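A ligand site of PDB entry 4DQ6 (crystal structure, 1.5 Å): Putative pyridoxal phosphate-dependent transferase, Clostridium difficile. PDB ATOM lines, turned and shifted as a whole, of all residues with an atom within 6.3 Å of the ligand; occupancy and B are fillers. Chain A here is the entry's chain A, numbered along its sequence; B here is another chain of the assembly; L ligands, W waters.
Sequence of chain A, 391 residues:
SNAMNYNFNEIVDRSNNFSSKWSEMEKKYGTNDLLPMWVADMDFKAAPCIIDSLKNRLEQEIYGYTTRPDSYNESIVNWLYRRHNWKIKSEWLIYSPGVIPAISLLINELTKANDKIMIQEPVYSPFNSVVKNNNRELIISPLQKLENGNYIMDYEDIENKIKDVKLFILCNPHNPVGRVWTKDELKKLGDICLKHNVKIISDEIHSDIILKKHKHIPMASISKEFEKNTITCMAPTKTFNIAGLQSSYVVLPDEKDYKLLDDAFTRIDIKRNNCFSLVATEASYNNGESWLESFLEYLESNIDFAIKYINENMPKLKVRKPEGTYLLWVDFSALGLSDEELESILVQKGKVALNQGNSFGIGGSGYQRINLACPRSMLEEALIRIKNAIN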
ATOM      1  N   ALA A  40     -17.972  18.313  20.090  1.00  0.00           N
ATOM      2  CA  ALA A  40     -17.848  18.558  18.648  1.00  0.00           C
ATOM      3  C   ALA A  40     -16.474  19.096  18.249  1.00  0.00           C
ATOM      4  O   ALA A  40     -16.316  20.274  17.878  1.00  0.00           O
ATOM      5  CB  ALA A  40     -18.988  19.530  18.211  1.00  0.00           C
ATOM      6  N   PRO A  97     -12.420  35.474  19.350  1.00  0.00           N
ATOM      7  CA  PRO A  97     -11.795  34.145  19.598  1.00  0.00           C
ATOM      8  C   PRO A  97     -12.798  33.003  19.472  1.00  0.00           C
ATOM      9  O   PRO A  97     -12.436  31.848  19.383  1.00  0.00           O
ATOM     10  CB  PRO A  97     -11.207  34.272  20.985  1.00  0.00           C
ATOM     11  CG  PRO A  97     -11.920  35.383  21.578  1.00  0.00           C
ATOM     12  CD  PRO A  97     -12.296  36.362  20.504  1.00  0.00           C
ATOM     13  N   GLY A  98     -14.066  33.305  19.587  1.00  0.00           N
ATOM     14  CA  GLY A  98     -15.157  32.326  19.480  1.00  0.00           C
ATOM     15  C   GLY A  98     -16.508  32.921  19.195  1.00  0.00           C
ATOM     16  O   GLY A  98     -16.792  34.144  19.388  1.00  0.00           O
ATOM     17  N   VAL A  99     -17.412  32.057  18.772  1.00  0.00           N
ATOM     18  CA  VAL A  99     -18.775  32.490  18.491  1.00  0.00           C
ATOM     19  C   VAL A  99     -19.463  32.934  19.739  1.00  0.00           C
ATOM     20  O   VAL A  99     -20.101  33.990  19.717  1.00  0.00           O
ATOM     21  CB  VAL A  99     -19.552  31.368  17.781  1.00  0.00           C
ATOM     22  CG1 VAL A  99     -21.042  31.683  17.711  1.00  0.00           C
ATOM     23  CG2 VAL A  99     -18.945  31.186  16.374  1.00  0.00           C
ATOM     24  N   ILE A 100     -19.415  32.154  20.813  1.00  0.00           N
ATOM     25  CA  ILE A 100     -20.195  32.555  21.993  1.00  0.00           C
ATOM     26  C   ILE A 100     -19.696  33.840  22.647  1.00  0.00           C
ATOM     27  O   ILE A 100     -20.474  34.713  23.029  1.00  0.00           O
ATOM     28  CB  ILE A 100     -20.303  31.393  22.979  1.00  0.00           C
ATOM     29  CG1 ILE A 100     -21.032  30.245  22.289  1.00  0.00           C
ATOM     30  CG2 ILE A 100     -21.034  31.870  24.254  1.00  0.00           C
ATOM     31  CD1 ILE A 100     -22.466  30.520  21.867  1.00  0.00           C
ATOM     32  N   PRO A 101     -18.374  34.102  22.682  1.00  0.00           N
ATOM     33  CA  PRO A 101     -17.913  35.377  23.153  1.00  0.00           C
ATOM     34  C   PRO A 101     -18.516  36.556  22.389  1.00  0.00           C
ATOM     35  O   PRO A 101     -18.921  37.556  22.979  1.00  0.00           O
ATOM     36  CB  PRO A 101     -16.415  35.323  22.893  1.00  0.00           C
ATOM     37  CG  PRO A 101     -16.051  33.887  22.997  1.00  0.00           C
ATOM     38  CD  PRO A 101     -17.272  33.116  22.587  1.00  0.00           C
ATOM     39  N   VAL A 123     -31.399  23.024  21.361  1.00  0.00           N
ATOM     40  CA  VAL A 123     -30.327  23.686  20.672  1.00  0.00           C
ATOM     41  C   VAL A 123     -29.095  23.674  21.568  1.00  0.00           C
ATOM     42  O   VAL A 123     -29.203  23.563  22.781  1.00  0.00           O
ATOM     43  CB  VAL A 123     -30.711  25.125  20.199  1.00  0.00           C
ATOM     44  CG1 VAL A 123     -30.820  26.065  21.414  1.00  0.00           C
ATOM     45  CG2 VAL A 123     -29.726  25.718  19.192  1.00  0.00           C
ATOM     46  N   TYR A 124     -27.959  23.826  20.914  1.00  0.00           N
ATOM     47  CA  TYR A 124     -26.592  24.072  21.482  1.00  0.00           C
ATOM     48  C   TYR A 124     -26.751  24.821  22.807  1.00  0.00           C
ATOM     49  O   TYR A 124     -27.333  25.905  22.839  1.00  0.00           O
ATOM     50  CB  TYR A 124     -25.820  24.895  20.482  1.00  0.00           C
ATOM     51  CG  TYR A 124     -24.379  25.125  20.853  1.00  0.00           C
ATOM     52  CD1 TYR A 124     -23.543  24.071  21.139  1.00  0.00           C
ATOM     53  CD2 TYR A 124     -23.858  26.422  20.881  1.00  0.00           C
ATOM     54  CE1 TYR A 124     -22.236  24.271  21.492  1.00  0.00           C
ATOM     55  CE2 TYR A 124     -22.502  26.639  21.224  1.00  0.00           C
ATOM     56  CZ  TYR A 124     -21.724  25.543  21.537  1.00  0.00           C
ATOM     57  OH  TYR A 124     -20.370  25.668  21.879  1.00  0.00           O
ATOM     58  N   PHE A 127     -26.444  28.651  23.936  1.00  0.00           N
ATOM     59  CA  PHE A 127     -27.515  29.616  23.549  1.00  0.00           C
ATOM     60  C   PHE A 127     -28.394  30.028  24.760  1.00  0.00           C
ATOM     61  O   PHE A 127     -28.785  31.189  24.907  1.00  0.00           O
ATOM     62  CB  PHE A 127     -28.440  29.045  22.490  1.00  0.00           C
ATOM     63  CG  PHE A 127     -27.965  29.222  21.059  1.00  0.00           C
ATOM     64  CD1 PHE A 127     -26.654  29.274  20.711  1.00  0.00           C
ATOM     65  CD2 PHE A 127     -28.953  29.317  20.087  1.00  0.00           C
ATOM     66  CE1 PHE A 127     -26.309  29.434  19.364  1.00  0.00           C
ATOM     67  CE2 PHE A 127     -28.643  29.498  18.771  1.00  0.00           C
ATOM     68  CZ  PHE A 127     -27.318  29.500  18.394  1.00  0.00           C
ATOM     69  N   CYS A 171     -29.840  29.218  15.018  1.00  0.00           N
ATOM     70  CA  CYS A 171     -28.774  28.286  14.690  1.00  0.00           C
ATOM     71  C   CYS A 171     -28.992  27.710  13.299  1.00  0.00           C
ATOM     72  O   CYS A 171     -30.000  27.084  13.066  1.00  0.00           O
ATOM     73  CB  CYS A 171     -28.770  27.172  15.749  1.00  0.00           C
ATOM     74  SG  CYS A 171     -27.234  26.254  15.919  1.00  0.00           S
ATOM     75  N   PRO A 173     -26.648  25.881  10.131  1.00  0.00           N
ATOM     76  CA  PRO A 173     -27.477  24.732  10.485  1.00  0.00           C
ATOM     77  C   PRO A 173     -27.748  24.577  11.985  1.00  0.00           C
ATOM     78  O   PRO A 173     -26.941  25.035  12.820  1.00  0.00           O
ATOM     79  CB  PRO A 173     -26.663  23.521   9.994  1.00  0.00           C
ATOM     80  CG  PRO A 173     -25.707  24.077   9.008  1.00  0.00           C
ATOM     81  CD  PRO A 173     -25.425  25.481   9.398  1.00  0.00           C
ATOM     82  N   ASN A 175     -27.833  22.780  15.341  1.00  0.00           N
ATOM     83  CA  ASN A 175     -27.293  21.740  16.237  1.00  0.00           C
ATOM     84  C   ASN A 175     -28.193  21.657  17.466  1.00  0.00           C
ATOM     85  O   ASN A 175     -28.393  22.679  18.125  1.00  0.00           O
ATOM     86  CB  ASN A 175     -25.861  22.162  16.603  1.00  0.00           C
ATOM     87  CG  ASN A 175     -25.304  21.473  17.806  1.00  0.00           C
ATOM     88  OD1 ASN A 175     -25.765  20.451  18.248  1.00  0.00           O
ATOM     89  ND2 ASN A 175     -24.183  22.050  18.320  1.00  0.00           N
ATOM     90  N   ASP A 203     -26.047  32.124  14.192  1.00  0.00           N
ATOM     91  CA  ASP A 203     -24.869  31.327  14.385  1.00  0.00           C
ATOM     92  C   ASP A 203     -24.807  30.286  13.266  1.00  0.00           C
ATOM     93  O   ASP A 203     -25.506  29.277  13.296  1.00  0.00           O
ATOM     94  CB  ASP A 203     -24.945  30.663  15.768  1.00  0.00           C
ATOM     95  CG  ASP A 203     -23.800  29.773  16.091  1.00  0.00           C
ATOM     96  OD1 ASP A 203     -22.967  29.505  15.230  1.00  0.00           O
ATOM     97  OD2 ASP A 203     -23.710  29.364  17.267  1.00  0.00           O
ATOM     98  N   ILE A 205     -22.036  28.641  12.431  1.00  0.00           N
ATOM     99  CA  ILE A 205     -20.717  28.042  12.537  1.00  0.00           C
ATOM    100  C   ILE A 205     -20.662  26.706  11.744  1.00  0.00           C
ATOM    101  O   ILE A 205     -19.579  26.321  11.243  1.00  0.00           O
ATOM    102  CB  ILE A 205     -20.251  27.848  13.970  1.00  0.00           C
ATOM    103  CG1 ILE A 205     -18.710  27.546  14.014  1.00  0.00           C
ATOM    104  CG2 ILE A 205     -21.009  26.741  14.629  1.00  0.00           C
ATOM    105  CD1 ILE A 205     -18.133  27.532  15.423  1.00  0.00           C
ATOM    106  N   HIS A 206     -21.747  25.973  11.613  1.00  0.00           N
ATOM    107  CA  HIS A 206     -21.707  24.674  10.864  1.00  0.00           C
ATOM    108  C   HIS A 206     -21.953  24.834   9.372  1.00  0.00           C
ATOM    109  O   HIS A 206     -22.245  23.851   8.673  1.00  0.00           O
ATOM    110  CB  HIS A 206     -22.700  23.658  11.421  1.00  0.00           C
ATOM    111  CG  HIS A 206     -22.515  23.312  12.868  1.00  0.00           C
ATOM    112  ND1 HIS A 206     -21.702  22.248  13.263  1.00  0.00           N
ATOM    113  CD2 HIS A 206     -22.978  23.924  14.019  1.00  0.00           C
ATOM    114  CE1 HIS A 206     -21.712  22.190  14.607  1.00  0.00           C
ATOM    115  NE2 HIS A 206     -22.474  23.227  15.081  1.00  0.00           N
ATOM    116  N   ALA A 235     -16.953  30.604  11.396  1.00  0.00           N
ATOM    117  CA  ALA A 235     -15.598  30.345  11.855  1.00  0.00           C
ATOM    118  C   ALA A 235     -15.069  29.227  10.981  1.00  0.00           C
ATOM    119  O   ALA A 235     -15.855  28.465  10.439  1.00  0.00           O
ATOM    120  CB  ALA A 235     -15.578  29.864  13.296  1.00  0.00           C
ATOM    121  N   THR A 237     -13.437  26.839  12.475  1.00  0.00           N
ATOM    122  CA  THR A 237     -13.067  25.894  13.500  1.00  0.00           C
ATOM    123  C   THR A 237     -13.813  24.569  13.398  1.00  0.00           C
ATOM    124  O   THR A 237     -13.215  23.525  13.589  1.00  0.00           O
ATOM    125  CB  THR A 237     -13.191  26.436  14.911  1.00  0.00           C
ATOM    126  OG1 THR A 237     -14.504  26.934  15.049  1.00  0.00           O
ATOM    127  CG2 THR A 237     -12.212  27.557  15.137  1.00  0.00           C
ATOM    128  N   LYS A 238     -15.110  24.601  13.221  1.00  0.00           N
ATOM    129  CA  LYS A 238     -15.904  23.354  13.106  1.00  0.00           C
ATOM    130  C   LYS A 238     -15.516  22.698  11.780  1.00  0.00           C
ATOM    131  O   LYS A 238     -15.285  21.484  11.738  1.00  0.00           O
ATOM    132  CB  LYS A 238     -17.406  23.561  13.127  1.00  0.00           C
ATOM    133  CG  LYS A 238     -17.936  23.955  14.485  1.00  0.00           C
ATOM    134  CD  LYS A 238     -18.101  22.745  15.440  1.00  0.00           C
ATOM    135  CE  LYS A 238     -18.033  23.124  16.930  1.00  0.00           C
ATOM    136  NZ  LYS A 238     -19.302  23.553  17.554  1.00  0.00           N
ATOM    137  N   ALA A 243     -10.565  24.185  16.436  1.00  0.00           N
ATOM    138  CA  ALA A 243     -11.167  24.918  17.621  1.00  0.00           C
ATOM    139  C   ALA A 243     -10.062  25.283  18.614  1.00  0.00           C
ATOM    140  O   ALA A 243     -10.143  26.301  19.288  1.00  0.00           O
ATOM    141  CB  ALA A 243     -12.258  24.106  18.311  1.00  0.00           C
ATOM    142  N   SER A 247     -10.415  30.879  16.460  1.00  0.00           N
ATOM    143  CA  SER A 247     -10.621  31.886  15.417  1.00  0.00           C
ATOM    144  C   SER A 247     -12.056  31.872  15.035  1.00  0.00           C
ATOM    145  O   SER A 247     -12.600  30.820  14.716  1.00  0.00           O
ATOM    146  CB  SER A 247      -9.805  31.477  14.192  1.00  0.00           C
ATOM    147  OG  SER A 247     -10.055  32.277  13.021  1.00  0.00           O
ATOM    148  N   SER A 248     -12.697  33.049  14.972  1.00  0.00           N
ATOM    149  CA  SER A 248     -14.026  33.142  14.423  1.00  0.00           C
ATOM    150  C   SER A 248     -14.191  34.588  13.952  1.00  0.00           C
ATOM    151  O   SER A 248     -13.331  35.454  14.149  1.00  0.00           O
ATOM    152  CB  SER A 248     -15.063  32.761  15.425  1.00  0.00           C
ATOM    153  OG  SER A 248     -15.235  33.775  16.384  1.00  0.00           O
ATOM    154  N   LEU A 327     -23.121  15.627  13.433  1.00  0.00           N
ATOM    155  CA  LEU A 327     -23.690  15.231  14.696  1.00  0.00           C
ATOM    156  C   LEU A 327     -24.991  14.490  14.414  1.00  0.00           C
ATOM    157  O   LEU A 327     -25.831  15.004  13.671  1.00  0.00           O
ATOM    158  CB  LEU A 327     -23.939  16.481  15.577  1.00  0.00           C
ATOM    159  CG  LEU A 327     -22.651  17.299  15.858  1.00  0.00           C
ATOM    160  CD1 LEU A 327     -23.032  18.692  16.448  1.00  0.00           C
ATOM    161  CD2 LEU A 327     -21.634  16.603  16.743  1.00  0.00           C
ATOM    162  N   ARG A 369     -26.952  12.804  21.438  1.00  0.00           N
ATOM    163  CA  ARG A 369     -26.157  13.274  20.303  1.00  0.00           C
ATOM    164  C   ARG A 369     -24.792  12.593  20.181  1.00  0.00           C
ATOM    165  O   ARG A 369     -24.030  12.511  21.140  1.00  0.00           O
ATOM    166  CB  ARG A 369     -25.986  14.789  20.386  1.00  0.00           C
ATOM    167  CG  ARG A 369     -25.650  15.461  19.088  1.00  0.00           C
ATOM    168  CD  ARG A 369     -25.066  16.850  19.278  1.00  0.00           C
ATOM    169  NE  ARG A 369     -23.736  16.859  19.903  1.00  0.00           N
ATOM    170  CZ  ARG A 369     -23.093  17.946  20.245  1.00  0.00           C
ATOM    171  NH1 ARG A 369     -23.659  19.169  20.065  1.00  0.00           N
ATOM    172  NH2 ARG A 369     -21.882  17.870  20.764  1.00  0.00           N
ATOM    173  N   TYR B  65     -10.387  21.148  20.833  1.00  0.00           N
ATOM    174  CA  TYR B  65     -10.498  21.796  22.112  1.00  0.00           C
ATOM    175  C   TYR B  65      -9.550  21.317  23.157  1.00  0.00           C
ATOM    176  O   TYR B  65      -9.352  20.104  23.329  1.00  0.00           O
ATOM    177  CB  TYR B  65     -11.937  21.594  22.642  1.00  0.00           C
ATOM    178  CG  TYR B  65     -13.033  22.337  21.887  1.00  0.00           C
ATOM    179  CD1 TYR B  65     -13.142  23.693  21.991  1.00  0.00           C
ATOM    180  CD2 TYR B  65     -13.888  21.667  21.037  1.00  0.00           C
ATOM    181  CE1 TYR B  65     -14.150  24.390  21.319  1.00  0.00           C
ATOM    182  CE2 TYR B  65     -14.894  22.369  20.317  1.00  0.00           C
ATOM    183  CZ  TYR B  65     -15.005  23.696  20.475  1.00  0.00           C
ATOM    184  OH  TYR B  65     -15.947  24.412  19.770  1.00  0.00           O
ATOM    185  N   ASP B 269     -17.558  33.393  27.827  1.00  0.00           N
ATOM    186  CA  ASP B 269     -17.121  32.088  27.329  1.00  0.00           C
ATOM    187  C   ASP B 269     -15.681  32.084  26.872  1.00  0.00           C
ATOM    188  O   ASP B 269     -15.352  31.601  25.800  1.00  0.00           O
ATOM    189  CB  ASP B 269     -18.045  31.529  26.256  1.00  0.00           C
ATOM    190  CG  ASP B 269     -17.720  30.090  25.902  1.00  0.00           C
ATOM    191  OD1 ASP B 269     -17.394  29.284  26.821  1.00  0.00           O
ATOM    192  OD2 ASP B 269     -17.730  29.780  24.687  1.00  0.00           O
HETATM  193  N1  LIG L   1     -22.115  27.526  17.897  1.00  0.00           N
HETATM  194  C1  LIG L   1     -22.602  26.261  17.660  1.00  0.00           C
HETATM  195  C2  LIG L   1     -23.978  25.975  17.149  1.00  0.00           C
HETATM  196  C3  LIG L   1     -21.774  25.098  17.889  1.00  0.00           C
HETATM  197  O1  LIG L   1     -22.240  23.876  17.678  1.00  0.00           O
HETATM  198  C4  LIG L   1     -20.414  25.294  18.375  1.00  0.00           C
HETATM  199  C5  LIG L   1     -19.518  24.115  18.686  1.00  0.00           C
HETATM  200  C6  LIG L   1     -19.974  26.661  18.592  1.00  0.00           C
HETATM  201  C7  LIG L   1     -20.861  27.740  18.352  1.00  0.00           C
HETATM  202  C8  LIG L   1     -18.571  26.876  19.055  1.00  0.00           C
HETATM  203  O2  LIG L   1     -18.589  28.111  19.695  1.00  0.00           O
HETATM  204  P1  LIG L   1     -17.137  28.731  20.050  1.00  0.00           P
HETATM  205  O3  LIG L   1     -16.628  29.270  18.763  1.00  0.00           O
HETATM  206  O4  LIG L   1     -17.566  29.788  21.154  1.00  0.00           O
HETATM  207  O5  LIG L   1     -16.316  27.491  20.517  1.00  0.00           O
HETATM  208  O   HOH W   1     -21.763  21.418  19.498  1.00  0.00           O
HETATM  209  O   HOH W   2     -15.081  29.199  16.577  1.00  0.00           O
HETATM  210  O   HOH W   3     -19.079  27.809  22.944  1.00  0.00           O
HETATM  211  O   HOH W   4     -18.547  23.250  21.774  1.00  0.00           O
HETATM  212  O   HOH W   5     -16.805  26.218  22.599  1.00  0.00           O
HETATM  213  O   HOH W   6     -15.517  30.428  22.974  1.00  0.00           O
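Water W5 bridges O5 of the ligand (2.5 Å) and OH of Tyr 65 of chain B (3.5 Å).
Water W2 lies within hydrogen-bond range of an oxygen (O3) of the ligand (2.7 Å), the side-chain hydroxyl of Thr 237 (2.8 Å) and the backbone carbonyl oxygen of Ser 247 (3.5 Å).
Water W6 bridges an oxygen (O4) of the ligand and the side-chain carboxylate (OD2) of Asp 269 of chain B.
Water W3 lies within hydrogen-bond range of the side-chain hydroxyl (OH) of Tyr 124 (2.7 Å), the side-chain carboxylate (OD2) of Asp 269 of chain B (3.0 Å) and an oxygen (O4) of the ligand (3.1 Å).
Water W1 lies within hydrogen-bond range of ND2 of Asn 175, NH1 of Arg 369 and O1 of the ligand.
Water W4 bridges OH of Tyr 124 and OH of Tyr 65 of chain B.
Residues that only touch the ligand: Tyr 124, Ile 205, Gly 98, Cys 171, Asp 269 of chain B and Pro 101.
Hydrophobic or aromatic side chains within 4 Å of the ligand: Val 99, Ile 100, Pro 101, Tyr 124, Ile 205, His 206 and Tyr 65 of chain B.
Within 4 Å of the ligand: Gly 98, Val 99, Ile 100, Pro 101, Tyr 124, Cys 171, Asn 175, Asp 203, Ile 205, His 206, Lys 238, Tyr 65 of chain B and Asp 269 of chain B.
The nearest printed residue that does not touch the ligand is Ala 40 (4.6 Å).
The side-chain amino group of Lys 238 is covalently linked to a carbon (C5) of the ligand.
OD2 of Asp 203 lies within hydrogen-bond range of N1 of the ligand, at 2.5 Å.
A ring nitrogen (NE2) of His 206 sits at hydrogen-bond distance from an oxygen (O1) of the ligand, at 2.7 Å.
The side-chain amide nitrogen of Asn 175 is in hydrogen-bond range of an oxygen (O1) of the ligand (2.7 Å).
O3 of the ligand is in hydrogen-bond range of N of Val 99 (2.9 Å).
N of Ile 100 is in hydrogen-bond range of O4 of the ligand.
OH of Tyr 65 of chain B lies within hydrogen-bond range of O5 of the ligand.
N of Ile 205 is in hydrogen-bond range of OD1 of Asp 203, at 3.1 Å.
The backbone carbonyl oxygen of Asn 175 is in hydrogen-bond range of the backbone NH of Tyr 124, at 3.0 Å.
N of Asn 175 sits at hydrogen-bond distance from SG of Cys 171, at 3.6 Å.
The guanidinium group (NH1) of Arg 369 is in hydrogen-bond range of the side-chain amide oxygen (OD1) of Asn 175, 3.1 Å away.
O of Gly 98 sits close to OG of Ser 248 (3.4 Å).
The side-chain sulfur of Cys 171 is in hydrogen-bond range of the backbone carbonyl oxygen of Pro 173, at 3.3 Å.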
